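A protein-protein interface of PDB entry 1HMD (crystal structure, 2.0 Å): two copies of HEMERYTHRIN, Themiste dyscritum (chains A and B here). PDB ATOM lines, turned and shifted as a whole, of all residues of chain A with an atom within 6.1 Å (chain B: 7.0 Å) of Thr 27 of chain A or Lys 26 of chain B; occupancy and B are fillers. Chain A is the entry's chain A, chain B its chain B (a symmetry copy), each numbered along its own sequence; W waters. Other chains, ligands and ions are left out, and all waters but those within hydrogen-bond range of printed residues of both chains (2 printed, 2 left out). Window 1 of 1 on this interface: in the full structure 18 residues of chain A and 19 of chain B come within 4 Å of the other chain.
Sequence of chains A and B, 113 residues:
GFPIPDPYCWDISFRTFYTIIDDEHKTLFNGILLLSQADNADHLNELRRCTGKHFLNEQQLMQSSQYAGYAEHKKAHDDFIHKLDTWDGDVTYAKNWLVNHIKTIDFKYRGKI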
ATOM      1  N   ASP A  22      20.061 -17.706  -9.515  1.00  0.00           N
ATOM      2  CA  ASP A  22      20.180 -18.517 -10.737  1.00  0.00           C
ATOM      3  C   ASP A  22      21.661 -18.764 -11.069  1.00  0.00           C
ATOM      4  O   ASP A  22      21.992 -19.867 -11.496  1.00  0.00           O
ATOM      5  CB  ASP A  22      19.431 -17.909 -11.948  1.00  0.00           C
ATOM      6  CG  ASP A  22      17.922 -17.906 -11.743  1.00  0.00           C
ATOM      7  OD1 ASP A  22      17.353 -18.640 -10.923  1.00  0.00           O
ATOM      8  OD2 ASP A  22      17.316 -17.094 -12.481  1.00  0.00           O
ATOM      9  N   ASP A  23      22.475 -17.723 -11.007  1.00  0.00           N
ATOM     10  CA  ASP A  23      23.932 -17.872 -11.314  1.00  0.00           C
ATOM     11  C   ASP A  23      24.551 -18.821 -10.319  1.00  0.00           C
ATOM     12  O   ASP A  23      25.367 -19.639 -10.767  1.00  0.00           O
ATOM     13  CB  ASP A  23      24.635 -16.544 -11.412  1.00  0.00           C
ATOM     14  CG  ASP A  23      24.250 -15.759 -12.634  1.00  0.00           C
ATOM     15  OD1 ASP A  23      24.528 -14.546 -12.707  1.00  0.00           O
ATOM     16  OD2 ASP A  23      23.625 -16.366 -13.548  1.00  0.00           O
ATOM     17  N   GLU A  24      24.179 -18.763  -9.053  1.00  0.00           N
ATOM     18  CA  GLU A  24      24.758 -19.761  -8.128  1.00  0.00           C
ATOM     19  C   GLU A  24      24.303 -21.150  -8.422  1.00  0.00           C
ATOM     20  O   GLU A  24      25.069 -22.152  -8.321  1.00  0.00           O
ATOM     21  CB  GLU A  24      24.407 -19.398  -6.653  1.00  0.00           C
ATOM     22  CG  GLU A  24      25.124 -18.097  -6.215  1.00  0.00           C
ATOM     23  CD  GLU A  24      24.902 -17.645  -4.799  1.00  0.00           C
ATOM     24  OE1 GLU A  24      25.666 -16.810  -4.299  1.00  0.00           O
ATOM     25  OE2 GLU A  24      23.928 -18.151  -4.216  1.00  0.00           O
ATOM     26  N   HIS A  25      23.020 -21.296  -8.790  1.00  0.00           N
ATOM     27  CA  HIS A  25      22.497 -22.647  -9.101  1.00  0.00           C
ATOM     28  C   HIS A  25      23.276 -23.342 -10.228  1.00  0.00           C
ATOM     29  O   HIS A  25      23.493 -24.559 -10.139  1.00  0.00           O
ATOM     30  CB  HIS A  25      20.990 -22.658  -9.467  1.00  0.00           C
ATOM     31  CG  HIS A  25      20.098 -22.471  -8.277  1.00  0.00           C
ATOM     32  ND1 HIS A  25      18.785 -22.047  -8.431  1.00  0.00           N
ATOM     33  CD2 HIS A  25      20.280 -22.668  -6.948  1.00  0.00           C
ATOM     34  CE1 HIS A  25      18.214 -22.058  -7.236  1.00  0.00           C
ATOM     35  NE2 HIS A  25      19.108 -22.327  -6.300  1.00  0.00           N
ATOM     36  N   LYS A  26      23.628 -22.601 -11.236  1.00  0.00           N
ATOM     37  CA  LYS A  26      24.428 -23.092 -12.368  1.00  0.00           C
ATOM     38  C   LYS A  26      25.708 -23.741 -11.864  1.00  0.00           C
ATOM     39  O   LYS A  26      26.175 -24.738 -12.444  1.00  0.00           O
ATOM     40  CB  LYS A  26      24.734 -21.956 -13.343  1.00  0.00           C
ATOM     41  CG  LYS A  26      23.483 -21.389 -14.046  1.00  0.00           C
ATOM     42  CD  LYS A  26      23.791 -20.086 -14.762  1.00  0.00           C
ATOM     43  CE  LYS A  26      22.507 -19.364 -15.143  1.00  0.00           C
ATOM     44  NZ  LYS A  26      22.800 -18.056 -15.760  1.00  0.00           N
ATOM     45  N   THR A  27      26.266 -23.233 -10.759  1.00  0.00           N
ATOM     46  CA  THR A  27      27.517 -23.787 -10.231  1.00  0.00           C
ATOM     47  C   THR A  27      27.206 -25.095  -9.561  1.00  0.00           C
ATOM     48  O   THR A  27      28.101 -25.960  -9.526  1.00  0.00           O
ATOM     49  CB  THR A  27      28.339 -22.822  -9.295  1.00  0.00           C
ATOM     50  OG1 THR A  27      27.602 -22.744  -8.005  1.00  0.00           O
ATOM     51  CG2 THR A  27      28.592 -21.442  -9.835  1.00  0.00           C
ATOM     52  N   LEU A  28      26.003 -25.290  -9.033  1.00  0.00           N
ATOM     53  CA  LEU A  28      25.693 -26.570  -8.351  1.00  0.00           C
ATOM     54  C   LEU A  28      25.450 -27.648  -9.432  1.00  0.00           C
ATOM     55  O   LEU A  28      25.862 -28.801  -9.205  1.00  0.00           O
ATOM     56  CB  LEU A  28      24.605 -26.385  -7.357  1.00  0.00           C
ATOM     57  CG  LEU A  28      24.573 -25.310  -6.296  1.00  0.00           C
ATOM     58  CD1 LEU A  28      23.296 -25.355  -5.462  1.00  0.00           C
ATOM     59  CD2 LEU A  28      25.799 -25.523  -5.417  1.00  0.00           C
ATOM     60  N   PHE A  29      24.808 -27.295 -10.524  1.00  0.00           N
ATOM     61  CA  PHE A  29      24.608 -28.257 -11.636  1.00  0.00           C
ATOM     62  C   PHE A  29      25.987 -28.753 -12.115  1.00  0.00           C
ATOM     63  O   PHE A  29      26.258 -29.948 -12.241  1.00  0.00           O
ATOM     64  CB  PHE A  29      23.824 -27.645 -12.791  1.00  0.00           C
ATOM     65  CG  PHE A  29      22.331 -27.712 -12.587  1.00  0.00           C
ATOM     66  CD1 PHE A  29      21.690 -26.718 -11.832  1.00  0.00           C
ATOM     67  CD2 PHE A  29      21.630 -28.812 -13.068  1.00  0.00           C
ATOM     68  CE1 PHE A  29      20.321 -26.756 -11.655  1.00  0.00           C
ATOM     69  CE2 PHE A  29      20.239 -28.894 -12.888  1.00  0.00           C
ATOM     70  CZ  PHE A  29      19.617 -27.854 -12.184  1.00  0.00           C
ATOM     71  N   ASN A  30      26.844 -27.764 -12.336  1.00  0.00           N
ATOM     72  CA  ASN A  30      28.224 -28.055 -12.789  1.00  0.00           C
ATOM     73  C   ASN A  30      28.945 -28.956 -11.810  1.00  0.00           C
ATOM     74  O   ASN A  30      29.610 -29.909 -12.297  1.00  0.00           O
ATOM     75  CB  ASN A  30      28.986 -26.749 -13.078  1.00  0.00           C
ATOM     76  CG  ASN A  30      30.440 -27.011 -13.499  1.00  0.00           C
ATOM     77  OD1 ASN A  30      30.653 -27.363 -14.673  1.00  0.00           O
ATOM     78  ND2 ASN A  30      31.338 -26.938 -12.531  1.00  0.00           N
ATOM     79  N   GLY A  31      28.902 -28.694 -10.527  1.00  0.00           N
ATOM     80  CA  GLY A  31      29.608 -29.506  -9.509  1.00  0.00           C
ATOM     81  C   GLY A  31      29.133 -30.976  -9.596  1.00  0.00           C
ATOM     82  O   GLY A  31      29.974 -31.874  -9.473  1.00  0.00           O
ATOM     83  N   ILE A  32      27.834 -31.184  -9.760  1.00  0.00           N
ATOM     84  CA  ILE A  32      27.254 -32.530  -9.856  1.00  0.00           C
ATOM     85  C   ILE A  32      27.650 -33.156 -11.188  1.00  0.00           C
ATOM     86  O   ILE A  32      27.956 -34.357 -11.207  1.00  0.00           O
ATOM     87  CB  ILE A  32      25.729 -32.540  -9.579  1.00  0.00           C
ATOM     88  CG1 ILE A  32      25.476 -32.115  -8.107  1.00  0.00           C
ATOM     89  CG2 ILE A  32      25.080 -33.923  -9.848  1.00  0.00           C
ATOM     90  CD1 ILE A  32      23.942 -31.895  -7.810  1.00  0.00           C
ATOM     91  N   GLU A  46      34.920 -28.845  -5.161  1.00  0.00           N
ATOM     92  CA  GLU A  46      34.253 -27.806  -5.962  1.00  0.00           C
ATOM     93  C   GLU A  46      32.768 -27.696  -5.660  1.00  0.00           C
ATOM     94  O   GLU A  46      32.146 -26.651  -5.433  1.00  0.00           O
ATOM     95  CB  GLU A  46      34.436 -28.086  -7.452  1.00  0.00           C
ATOM     96  CG  GLU A  46      34.308 -26.878  -8.364  1.00  0.00           C
ATOM     97  CD  GLU A  46      35.245 -25.734  -8.194  1.00  0.00           C
ATOM     98  OE1 GLU A  46      35.031 -24.568  -8.477  1.00  0.00           O
ATOM     99  OE2 GLU A  46      36.366 -26.084  -7.771  1.00  0.00           O
ATOM    100  N   LEU A  47      32.075 -28.844  -5.714  1.00  0.00           N
ATOM    101  CA  LEU A  47      30.657 -28.845  -5.402  1.00  0.00           C
ATOM    102  C   LEU A  47      30.403 -28.411  -3.963  1.00  0.00           C
ATOM    103  O   LEU A  47      29.395 -27.703  -3.703  1.00  0.00           O
ATOM    104  CB  LEU A  47      30.070 -30.242  -5.710  1.00  0.00           C
ATOM    105  CG  LEU A  47      28.629 -30.480  -5.211  1.00  0.00           C
ATOM    106  CD1 LEU A  47      27.710 -29.508  -5.958  1.00  0.00           C
ATOM    107  CD2 LEU A  47      28.231 -31.919  -5.407  1.00  0.00           C
ATOM    108  N   ARG A  49      32.133 -26.564  -1.904  1.00  0.00           N
ATOM    109  CA  ARG A  49      32.358 -25.120  -1.718  1.00  0.00           C
ATOM    110  C   ARG A  49      31.146 -24.362  -2.288  1.00  0.00           C
ATOM    111  O   ARG A  49      30.551 -23.521  -1.601  1.00  0.00           O
ATOM    112  CB  ARG A  49      33.634 -24.629  -2.377  1.00  0.00           C
ATOM    113  CG  ARG A  49      33.871 -23.133  -2.310  1.00  0.00           C
ATOM    114  CD  ARG A  49      35.050 -22.736  -3.113  1.00  0.00           C
ATOM    115  NE  ARG A  49      34.966 -22.920  -4.556  1.00  0.00           N
ATOM    116  CZ  ARG A  49      34.269 -22.144  -5.396  1.00  0.00           C
ATOM    117  NH1 ARG A  49      34.287 -22.312  -6.724  1.00  0.00           N
ATOM    118  NH2 ARG A  49      33.499 -21.160  -4.906  1.00  0.00           N
ATOM    119  N   CYS A  50      30.804 -24.609  -3.540  1.00  0.00           N
ATOM    120  CA  CYS A  50      29.682 -23.903  -4.169  1.00  0.00           C
ATOM    121  C   CYS A  50      28.367 -24.103  -3.448  1.00  0.00           C
ATOM    122  O   CYS A  50      27.548 -23.143  -3.399  1.00  0.00           O
ATOM    123  CB  CYS A  50      29.586 -24.320  -5.644  1.00  0.00           C
ATOM    124  SG  CYS A  50      30.981 -23.715  -6.584  1.00  0.00           S
ATOM    125  N   THR A  51      28.100 -25.259  -2.932  1.00  0.00           N
ATOM    126  CA  THR A  51      26.890 -25.575  -2.176  1.00  0.00           C
ATOM    127  C   THR A  51      26.827 -24.801  -0.856  1.00  0.00           C
ATOM    128  O   THR A  51      25.808 -24.174  -0.484  1.00  0.00           O
ATOM    129  CB  THR A  51      26.736 -27.126  -1.949  1.00  0.00           C
ATOM    130  OG1 THR A  51      26.758 -27.734  -3.292  1.00  0.00           O
ATOM    131  CG2 THR A  51      25.455 -27.522  -1.195  1.00  0.00           C
ATOM    132  N   LYS A  53      28.392 -22.135  -0.017  1.00  0.00           N
ATOM    133  CA  LYS A  53      28.289 -20.707  -0.336  1.00  0.00           C
ATOM    134  C   LYS A  53      26.873 -20.358  -0.789  1.00  0.00           C
ATOM    135  O   LYS A  53      26.256 -19.373  -0.314  1.00  0.00           O
ATOM    136  CB  LYS A  53      29.295 -20.327  -1.404  1.00  0.00           C
ATOM    137  CG  LYS A  53      29.187 -18.885  -1.907  1.00  0.00           C
ATOM    138  CD  LYS A  53      30.114 -18.629  -3.083  1.00  0.00           C
ATOM    139  CE  LYS A  53      29.405 -18.399  -4.377  1.00  0.00           C
ATOM    140  NZ  LYS A  53      29.683 -19.395  -5.428  1.00  0.00           N
ATOM    141  N   HIS A  54      26.336 -21.148  -1.734  1.00  0.00           N
ATOM    142  CA  HIS A  54      24.989 -20.843  -2.232  1.00  0.00           C
ATOM    143  C   HIS A  54      23.971 -20.914  -1.079  1.00  0.00           C
ATOM    144  O   HIS A  54      23.147 -19.997  -0.901  1.00  0.00           O
ATOM    145  CB  HIS A  54      24.574 -21.758  -3.388  1.00  0.00           C
ATOM    146  CG  HIS A  54      23.105 -21.579  -3.702  1.00  0.00           C
ATOM    147  ND1 HIS A  54      22.600 -20.372  -4.088  1.00  0.00           N
ATOM    148  CD2 HIS A  54      22.065 -22.401  -3.489  1.00  0.00           C
ATOM    149  CE1 HIS A  54      21.275 -20.492  -4.175  1.00  0.00           C
ATOM    150  NE2 HIS A  54      20.941 -21.701  -3.814  1.00  0.00           N
ATOM    151  N   TYR B   8      29.691 -29.170 -23.442  1.00  0.00           N
ATOM    152  CA  TYR B   8      30.267 -27.848 -23.240  1.00  0.00           C
ATOM    153  C   TYR B   8      29.916 -27.273 -21.860  1.00  0.00           C
ATOM    154  O   TYR B   8      28.962 -26.519 -21.655  1.00  0.00           O
ATOM    155  CB  TYR B   8      29.817 -26.927 -24.363  1.00  0.00           C
ATOM    156  CG  TYR B   8      30.743 -25.739 -24.494  1.00  0.00           C
ATOM    157  CD1 TYR B   8      30.360 -24.530 -23.898  1.00  0.00           C
ATOM    158  CD2 TYR B   8      31.998 -25.868 -25.057  1.00  0.00           C
ATOM    159  CE1 TYR B   8      31.163 -23.417 -23.984  1.00  0.00           C
ATOM    160  CE2 TYR B   8      32.831 -24.756 -25.137  1.00  0.00           C
ATOM    161  CZ  TYR B   8      32.415 -23.540 -24.606  1.00  0.00           C
ATOM    162  OH  TYR B   8      33.226 -22.449 -24.702  1.00  0.00           O
ATOM    163  N   CYS B   9      30.756 -27.647 -20.946  1.00  0.00           N
ATOM    164  CA  CYS B   9      30.733 -27.338 -19.539  1.00  0.00           C
ATOM    165  C   CYS B   9      32.118 -27.155 -18.952  1.00  0.00           C
ATOM    166  O   CYS B   9      33.130 -27.645 -19.458  1.00  0.00           O
ATOM    167  CB  CYS B   9      29.934 -28.454 -18.830  1.00  0.00           C
ATOM    168  SG  CYS B   9      28.252 -27.809 -18.556  1.00  0.00           S
ATOM    169  N   TRP B  10      32.113 -26.275 -17.943  1.00  0.00           N
ATOM    170  CA  TRP B  10      33.367 -25.917 -17.252  1.00  0.00           C
ATOM    171  C   TRP B  10      34.012 -27.153 -16.672  1.00  0.00           C
ATOM    172  O   TRP B  10      33.293 -28.074 -16.190  1.00  0.00           O
ATOM    173  CB  TRP B  10      32.994 -24.851 -16.185  1.00  0.00           C
ATOM    174  CG  TRP B  10      34.172 -24.346 -15.385  1.00  0.00           C
ATOM    175  CD1 TRP B  10      34.881 -23.205 -15.691  1.00  0.00           C
ATOM    176  CD2 TRP B  10      34.731 -24.891 -14.206  1.00  0.00           C
ATOM    177  NE1 TRP B  10      35.836 -22.992 -14.718  1.00  0.00           N
ATOM    178  CE2 TRP B  10      35.776 -24.009 -13.800  1.00  0.00           C
ATOM    179  CE3 TRP B  10      34.502 -26.030 -13.435  1.00  0.00           C
ATOM    180  CZ2 TRP B  10      36.595 -24.251 -12.697  1.00  0.00           C
ATOM    181  CZ3 TRP B  10      35.264 -26.245 -12.323  1.00  0.00           C
ATOM    182  CH2 TRP B  10      36.299 -25.376 -11.953  1.00  0.00           C
ATOM    183  N   ASP B  11      35.331 -27.177 -16.586  1.00  0.00           N
ATOM    184  CA  ASP B  11      35.979 -28.348 -15.870  1.00  0.00           C
ATOM    185  C   ASP B  11      37.154 -27.756 -15.082  1.00  0.00           C
ATOM    186  O   ASP B  11      37.505 -26.578 -15.374  1.00  0.00           O
ATOM    187  CB  ASP B  11      36.220 -29.508 -16.810  1.00  0.00           C
ATOM    188  CG  ASP B  11      37.311 -29.313 -17.814  1.00  0.00           C
ATOM    189  OD1 ASP B  11      38.411 -28.921 -17.457  1.00  0.00           O
ATOM    190  OD2 ASP B  11      37.023 -29.431 -19.032  1.00  0.00           O
ATOM    191  N   THR B  19      38.193 -18.053  -6.977  1.00  0.00           N
ATOM    192  CA  THR B  19      36.892 -18.755  -6.896  1.00  0.00           C
ATOM    193  C   THR B  19      35.763 -17.940  -7.501  1.00  0.00           C
ATOM    194  O   THR B  19      34.916 -18.534  -8.214  1.00  0.00           O
ATOM    195  CB  THR B  19      36.495 -19.264  -5.449  1.00  0.00           C
ATOM    196  OG1 THR B  19      36.368 -18.049  -4.660  1.00  0.00           O
ATOM    197  CG2 THR B  19      37.448 -20.261  -4.802  1.00  0.00           C
ATOM    198  N   ILE B  21      35.940 -15.756  -9.934  1.00  0.00           N
ATOM    199  CA  ILE B  21      36.170 -15.819 -11.378  1.00  0.00           C
ATOM    200  C   ILE B  21      35.739 -17.193 -11.894  1.00  0.00           C
ATOM    201  O   ILE B  21      34.980 -17.260 -12.880  1.00  0.00           O
ATOM    202  CB  ILE B  21      37.647 -15.452 -11.729  1.00  0.00           C
ATOM    203  CG1 ILE B  21      37.961 -13.972 -11.395  1.00  0.00           C
ATOM    204  CG2 ILE B  21      37.991 -15.776 -13.210  1.00  0.00           C
ATOM    205  CD1 ILE B  21      37.221 -12.886 -12.144  1.00  0.00           C
ATOM    206  N   ASP B  22      36.195 -18.259 -11.241  1.00  0.00           N
ATOM    207  CA  ASP B  22      35.796 -19.602 -11.691  1.00  0.00           C
ATOM    208  C   ASP B  22      34.284 -19.744 -11.705  1.00  0.00           C
ATOM    209  O   ASP B  22      33.748 -20.377 -12.611  1.00  0.00           O
ATOM    210  CB  ASP B  22      36.461 -20.687 -10.822  1.00  0.00           C
ATOM    211  CG  ASP B  22      37.979 -20.700 -11.034  1.00  0.00           C
ATOM    212  OD1 ASP B  22      38.475 -20.169 -12.032  1.00  0.00           O
ATOM    213  OD2 ASP B  22      38.627 -21.352 -10.219  1.00  0.00           O
ATOM    214  N   ASP B  23      33.636 -19.300 -10.627  1.00  0.00           N
ATOM    215  CA  ASP B  23      32.157 -19.411 -10.537  1.00  0.00           C
ATOM    216  C   ASP B  23      31.494 -18.588 -11.623  1.00  0.00           C
ATOM    217  O   ASP B  23      30.487 -19.078 -12.187  1.00  0.00           O
ATOM    218  CB  ASP B  23      31.657 -19.085  -9.142  1.00  0.00           C
ATOM    219  CG  ASP B  23      31.932 -20.154  -8.145  1.00  0.00           C
ATOM    220  OD1 ASP B  23      31.777 -19.906  -6.922  1.00  0.00           O
ATOM    221  OD2 ASP B  23      32.381 -21.259  -8.528  1.00  0.00           O
ATOM    222  N   GLU B  24      31.982 -17.387 -11.929  1.00  0.00           N
ATOM    223  CA  GLU B  24      31.372 -16.665 -13.063  1.00  0.00           C
ATOM    224  C   GLU B  24      31.605 -17.355 -14.392  1.00  0.00           C
ATOM    225  O   GLU B  24      30.753 -17.309 -15.320  1.00  0.00           O
ATOM    226  CB  GLU B  24      31.908 -15.231 -13.139  1.00  0.00           C
ATOM    227  CG  GLU B  24      31.341 -14.398 -11.981  1.00  0.00           C
ATOM    228  CD  GLU B  24      31.880 -13.009 -11.834  1.00  0.00           C
ATOM    229  OE1 GLU B  24      31.405 -12.248 -10.996  1.00  0.00           O
ATOM    230  OE2 GLU B  24      32.842 -12.697 -12.564  1.00  0.00           O
ATOM    231  N   HIS B  25      32.793 -17.933 -14.570  1.00  0.00           N
ATOM    232  CA  HIS B  25      33.095 -18.667 -15.832  1.00  0.00           C
ATOM    233  C   HIS B  25      32.111 -19.793 -16.082  1.00  0.00           C
ATOM    234  O   HIS B  25      31.725 -20.041 -17.257  1.00  0.00           O
ATOM    235  CB  HIS B  25      34.558 -19.210 -15.860  1.00  0.00           C
ATOM    236  CG  HIS B  25      35.557 -18.129 -16.162  1.00  0.00           C
ATOM    237  ND1 HIS B  25      36.894 -18.340 -15.885  1.00  0.00           N
ATOM    238  CD2 HIS B  25      35.465 -16.891 -16.669  1.00  0.00           C
ATOM    239  CE1 HIS B  25      37.559 -17.269 -16.244  1.00  0.00           C
ATOM    240  NE2 HIS B  25      36.737 -16.351 -16.715  1.00  0.00           N
ATOM    241  N   LYS B  26      31.754 -20.557 -15.073  1.00  0.00           N
ATOM    242  CA  LYS B  26      30.782 -21.646 -15.144  1.00  0.00           C
ATOM    243  C   LYS B  26      29.471 -21.154 -15.777  1.00  0.00           C
ATOM    244  O   LYS B  26      28.860 -21.899 -16.573  1.00  0.00           O
ATOM    245  CB  LYS B  26      30.479 -22.279 -13.775  1.00  0.00           C
ATOM    246  CG  LYS B  26      31.706 -22.944 -13.153  1.00  0.00           C
ATOM    247  CD  LYS B  26      31.545 -23.299 -11.696  1.00  0.00           C
ATOM    248  CE  LYS B  26      32.866 -23.713 -11.055  1.00  0.00           C
ATOM    249  NZ  LYS B  26      32.651 -24.004  -9.604  1.00  0.00           N
ATOM    250  N   THR B  27      29.081 -19.909 -15.507  1.00  0.00           N
ATOM    251  CA  THR B  27      27.886 -19.338 -16.097  1.00  0.00           C
ATOM    252  C   THR B  27      28.061 -19.029 -17.578  1.00  0.00           C
ATOM    253  O   THR B  27      27.026 -19.009 -18.300  1.00  0.00           O
ATOM    254  CB  THR B  27      27.345 -18.069 -15.313  1.00  0.00           C
ATOM    255  OG1 THR B  27      28.190 -16.944 -15.664  1.00  0.00           O
ATOM    256  CG2 THR B  27      27.270 -18.303 -13.786  1.00  0.00           C
ATOM    257  N   LEU B  28      29.256 -18.708 -18.036  1.00  0.00           N
ATOM    258  CA  LEU B  28      29.480 -18.416 -19.470  1.00  0.00           C
ATOM    259  C   LEU B  28      29.409 -19.757 -20.229  1.00  0.00           C
ATOM    260  O   LEU B  28      28.862 -19.806 -21.331  1.00  0.00           O
ATOM    261  CB  LEU B  28      30.737 -17.623 -19.666  1.00  0.00           C
ATOM    262  CG  LEU B  28      31.118 -16.364 -18.976  1.00  0.00           C
ATOM    263  CD1 LEU B  28      32.012 -15.498 -19.889  1.00  0.00           C
ATOM    264  CD2 LEU B  28      29.929 -15.496 -18.618  1.00  0.00           C
ATOM    265  N   PHE B  29      30.019 -20.798 -19.668  1.00  0.00           N
ATOM    266  CA  PHE B  29      29.953 -22.128 -20.298  1.00  0.00           C
ATOM    267  C   PHE B  29      28.473 -22.517 -20.472  1.00  0.00           C
ATOM    268  O   PHE B  29      28.026 -23.032 -21.516  1.00  0.00           O
ATOM    269  CB  PHE B  29      30.690 -23.219 -19.521  1.00  0.00           C
ATOM    270  CG  PHE B  29      32.161 -23.303 -19.782  1.00  0.00           C
ATOM    271  CD1 PHE B  29      33.053 -22.494 -19.072  1.00  0.00           C
ATOM    272  CD2 PHE B  29      32.650 -24.196 -20.745  1.00  0.00           C
ATOM    273  CE1 PHE B  29      34.416 -22.537 -19.332  1.00  0.00           C
ATOM    274  CE2 PHE B  29      34.029 -24.281 -21.023  1.00  0.00           C
ATOM    275  CZ  PHE B  29      34.899 -23.431 -20.314  1.00  0.00           C
ATOM    276  N   ASN B  30      27.731 -22.364 -19.390  1.00  0.00           N
ATOM    277  CA  ASN B  30      26.284 -22.758 -19.436  1.00  0.00           C
ATOM    278  C   ASN B  30      25.558 -21.935 -20.487  1.00  0.00           C
ATOM    279  O   ASN B  30      24.686 -22.480 -21.186  1.00  0.00           O
ATOM    280  CB  ASN B  30      25.664 -22.674 -18.049  1.00  0.00           C
ATOM    281  CG  ASN B  30      24.150 -22.871 -18.043  1.00  0.00           C
ATOM    282  OD1 ASN B  30      23.693 -24.028 -18.034  1.00  0.00           O
ATOM    283  ND2 ASN B  30      23.404 -21.765 -18.113  1.00  0.00           N
ATOM    284  N   GLY B  31      25.825 -20.654 -20.549  1.00  0.00           N
ATOM    285  CA  GLY B  31      25.200 -19.742 -21.496  1.00  0.00           C
ATOM    286  C   GLY B  31      25.408 -20.254 -22.932  1.00  0.00           C
ATOM    287  O   GLY B  31      24.425 -20.249 -23.702  1.00  0.00           O
ATOM    288  N   ILE B 102      40.021 -17.889 -21.801  1.00  0.00           N
ATOM    289  CA  ILE B 102      40.399 -18.236 -20.422  1.00  0.00           C
ATOM    290  C   ILE B 102      41.829 -18.762 -20.338  1.00  0.00           C
ATOM    291  O   ILE B 102      42.615 -18.391 -19.460  1.00  0.00           O
ATOM    292  CB  ILE B 102      39.369 -19.250 -19.825  1.00  0.00           C
ATOM    293  CG1 ILE B 102      37.944 -18.638 -19.829  1.00  0.00           C
ATOM    294  CG2 ILE B 102      39.783 -19.755 -18.402  1.00  0.00           C
ATOM    295  CD1 ILE B 102      36.808 -19.673 -19.502  1.00  0.00           C
HETATM  296  O   HOH W   1      32.028 -17.329  -5.618  1.00  0.00           O
HETATM  297  O   HOH W   2      37.829 -23.550  -8.653  1.00  0.00           O
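OD2 of Asp 23 of chain B lies within hydrogen-bond range of SG of Cys 50 of chain A (3.4 Å).
NZ of Lys 53 of chain A is in salt-bridge range of OD1 of Asp 23 of chain B (2.6 Å).
The side-chain carboxylate (OE1) of Glu 46 of chain A is in salt-bridge range of the side-chain amino group (NZ) of Lys 26 of chain B (2.7 Å).
The side-chain carboxylate (OD2) of Asp 23 of chain B is in salt-bridge range of the guanidinium group (NH1) of Arg 49 of chain A (2.8 Å).
The side-chain amide oxygen (OD1) of Asn 30 of chain A sits close to the backbone carbonyl oxygen (O) of Trp 10 of chain B.
SG of Cys 50 of chain A sits at hydrogen-bond distance from NZ of Lys 26 of chain B (3.5 Å).
The side-chain sulfur of Cys 50 of chain A sits close to the side-chain hydroxyl of Thr 27 of chain A (3.8 Å).
OE1 of Glu 46 of chain A lies within salt-bridge range of NH1 of Arg 49 of chain A, at 3.0 Å.
The side-chain hydroxyl (OG1) of Thr 27 of chain B lies within hydrogen-bond range of the backbone carbonyl oxygen (O) of Glu 24 of chain B.
The side-chain amino group of Lys 26 of chain B lies within salt-bridge range of the side-chain carboxylate of Asp 23 of chain B (3.0 Å).
The backbone carbonyl oxygen of Glu 24 of chain A sits at hydrogen-bond distance from the side-chain hydroxyl of Thr 27 of chain A, at 2.6 Å.
The side-chain sulfur of Cys 50 of chain A lies within hydrogen-bond range of the backbone carbonyl oxygen of Glu 46 of chain A (3.4 Å).
Thr 27 of chain B touches Asp 23 of chain A (CG2 to O, 3.8 Å).
CD of Lys 26 of chain A touches ND2 of Asn 30 of chain B (3.8 Å).
CG2 of Thr 27 of chain A touches O of Asp 23 of chain B, at 3.8 Å.
Thr 27 of chain A touches Lys 26 of chain B.
Lys 26 of chain B touches Asn 30 of chain A.
Glu 46 of chain A touches Trp 10 of chain B (OE1 to CH2, 3.8 Å).
Thr 19 of chain B touches Arg 49 of chain A.
Arg 49 of chain A touches Lys 26 of chain B (NH1 to NZ, 3.7 Å).
Thr 27 of chain A touches two residues of chain B.
Of the printed residues of chain A, Lys 26 of chain B touches Thr 27 (3.95 Å), Asn 30 (3.7 Å), Glu 46 (2.7 Å), Arg 49 (3.7 Å) and Cys 50 (3.5 Å).
Printed residues of chain B within 4 Å of Lys 53 of chain A: Asp 23 (2.6 Å).
Of the printed residues of chain B, Asn 30 of chain A touches Trp 10 and Lys 26.
Of the printed residues of chain A, Asp 23 of chain B touches Thr 27, Arg 49, Cys 50 and Lys 53.
Printed residues of chain A within 4 Å of Asn 30 of chain B: Lys 26.
Of the printed residues of chain B, Glu 46 of chain A touches Trp 10 (3.8 Å) and Lys 26 (2.7 Å).
Ile 32 of chain A touches none of the printed residues of chain B.
The nearest residue of chain A that does not touch Lys 26 of chain B is Lys 26 of chain A (5.1 Å).
Of the 17 printed residues of chain B, 6 touch a printed residue of chain A.
Hydrophobic or aromatic side chains of chain B within 4 Å of the printed part of chain A: Trp 10.
Of the 18 printed residues of chain A, 8 touch a printed residue of chain B.
Asp 23 of chain A touches Thr 27 of chain B, and with the chains exchanged Thr 27 of chain A touches Asp 23 of chain B.
Lys 26 of chain A touches Asn 30 of chain B, and with the chains exchanged Asn 30 of chain A touches Lys 26 of chain B.
Thr 27 of chain A touches Lys 26 of chain B, but with the chains exchanged Lys 26 of chain A does not touch Thr 27 of chain B (4.03 Å).
Positions printed for both chains: 22, 23, 24, 25, 26, 27, 28, 29, 30 and 31.
Water W2 bridges OD2 of Asp 22 of chain B and OE1 of Glu 46 of chain A.
Water W1 lies within hydrogen-bond range of OD1 of Asp 23 of chain B (2.9 Å) and NZ of Lys 53 of chain A (3.1 Å).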
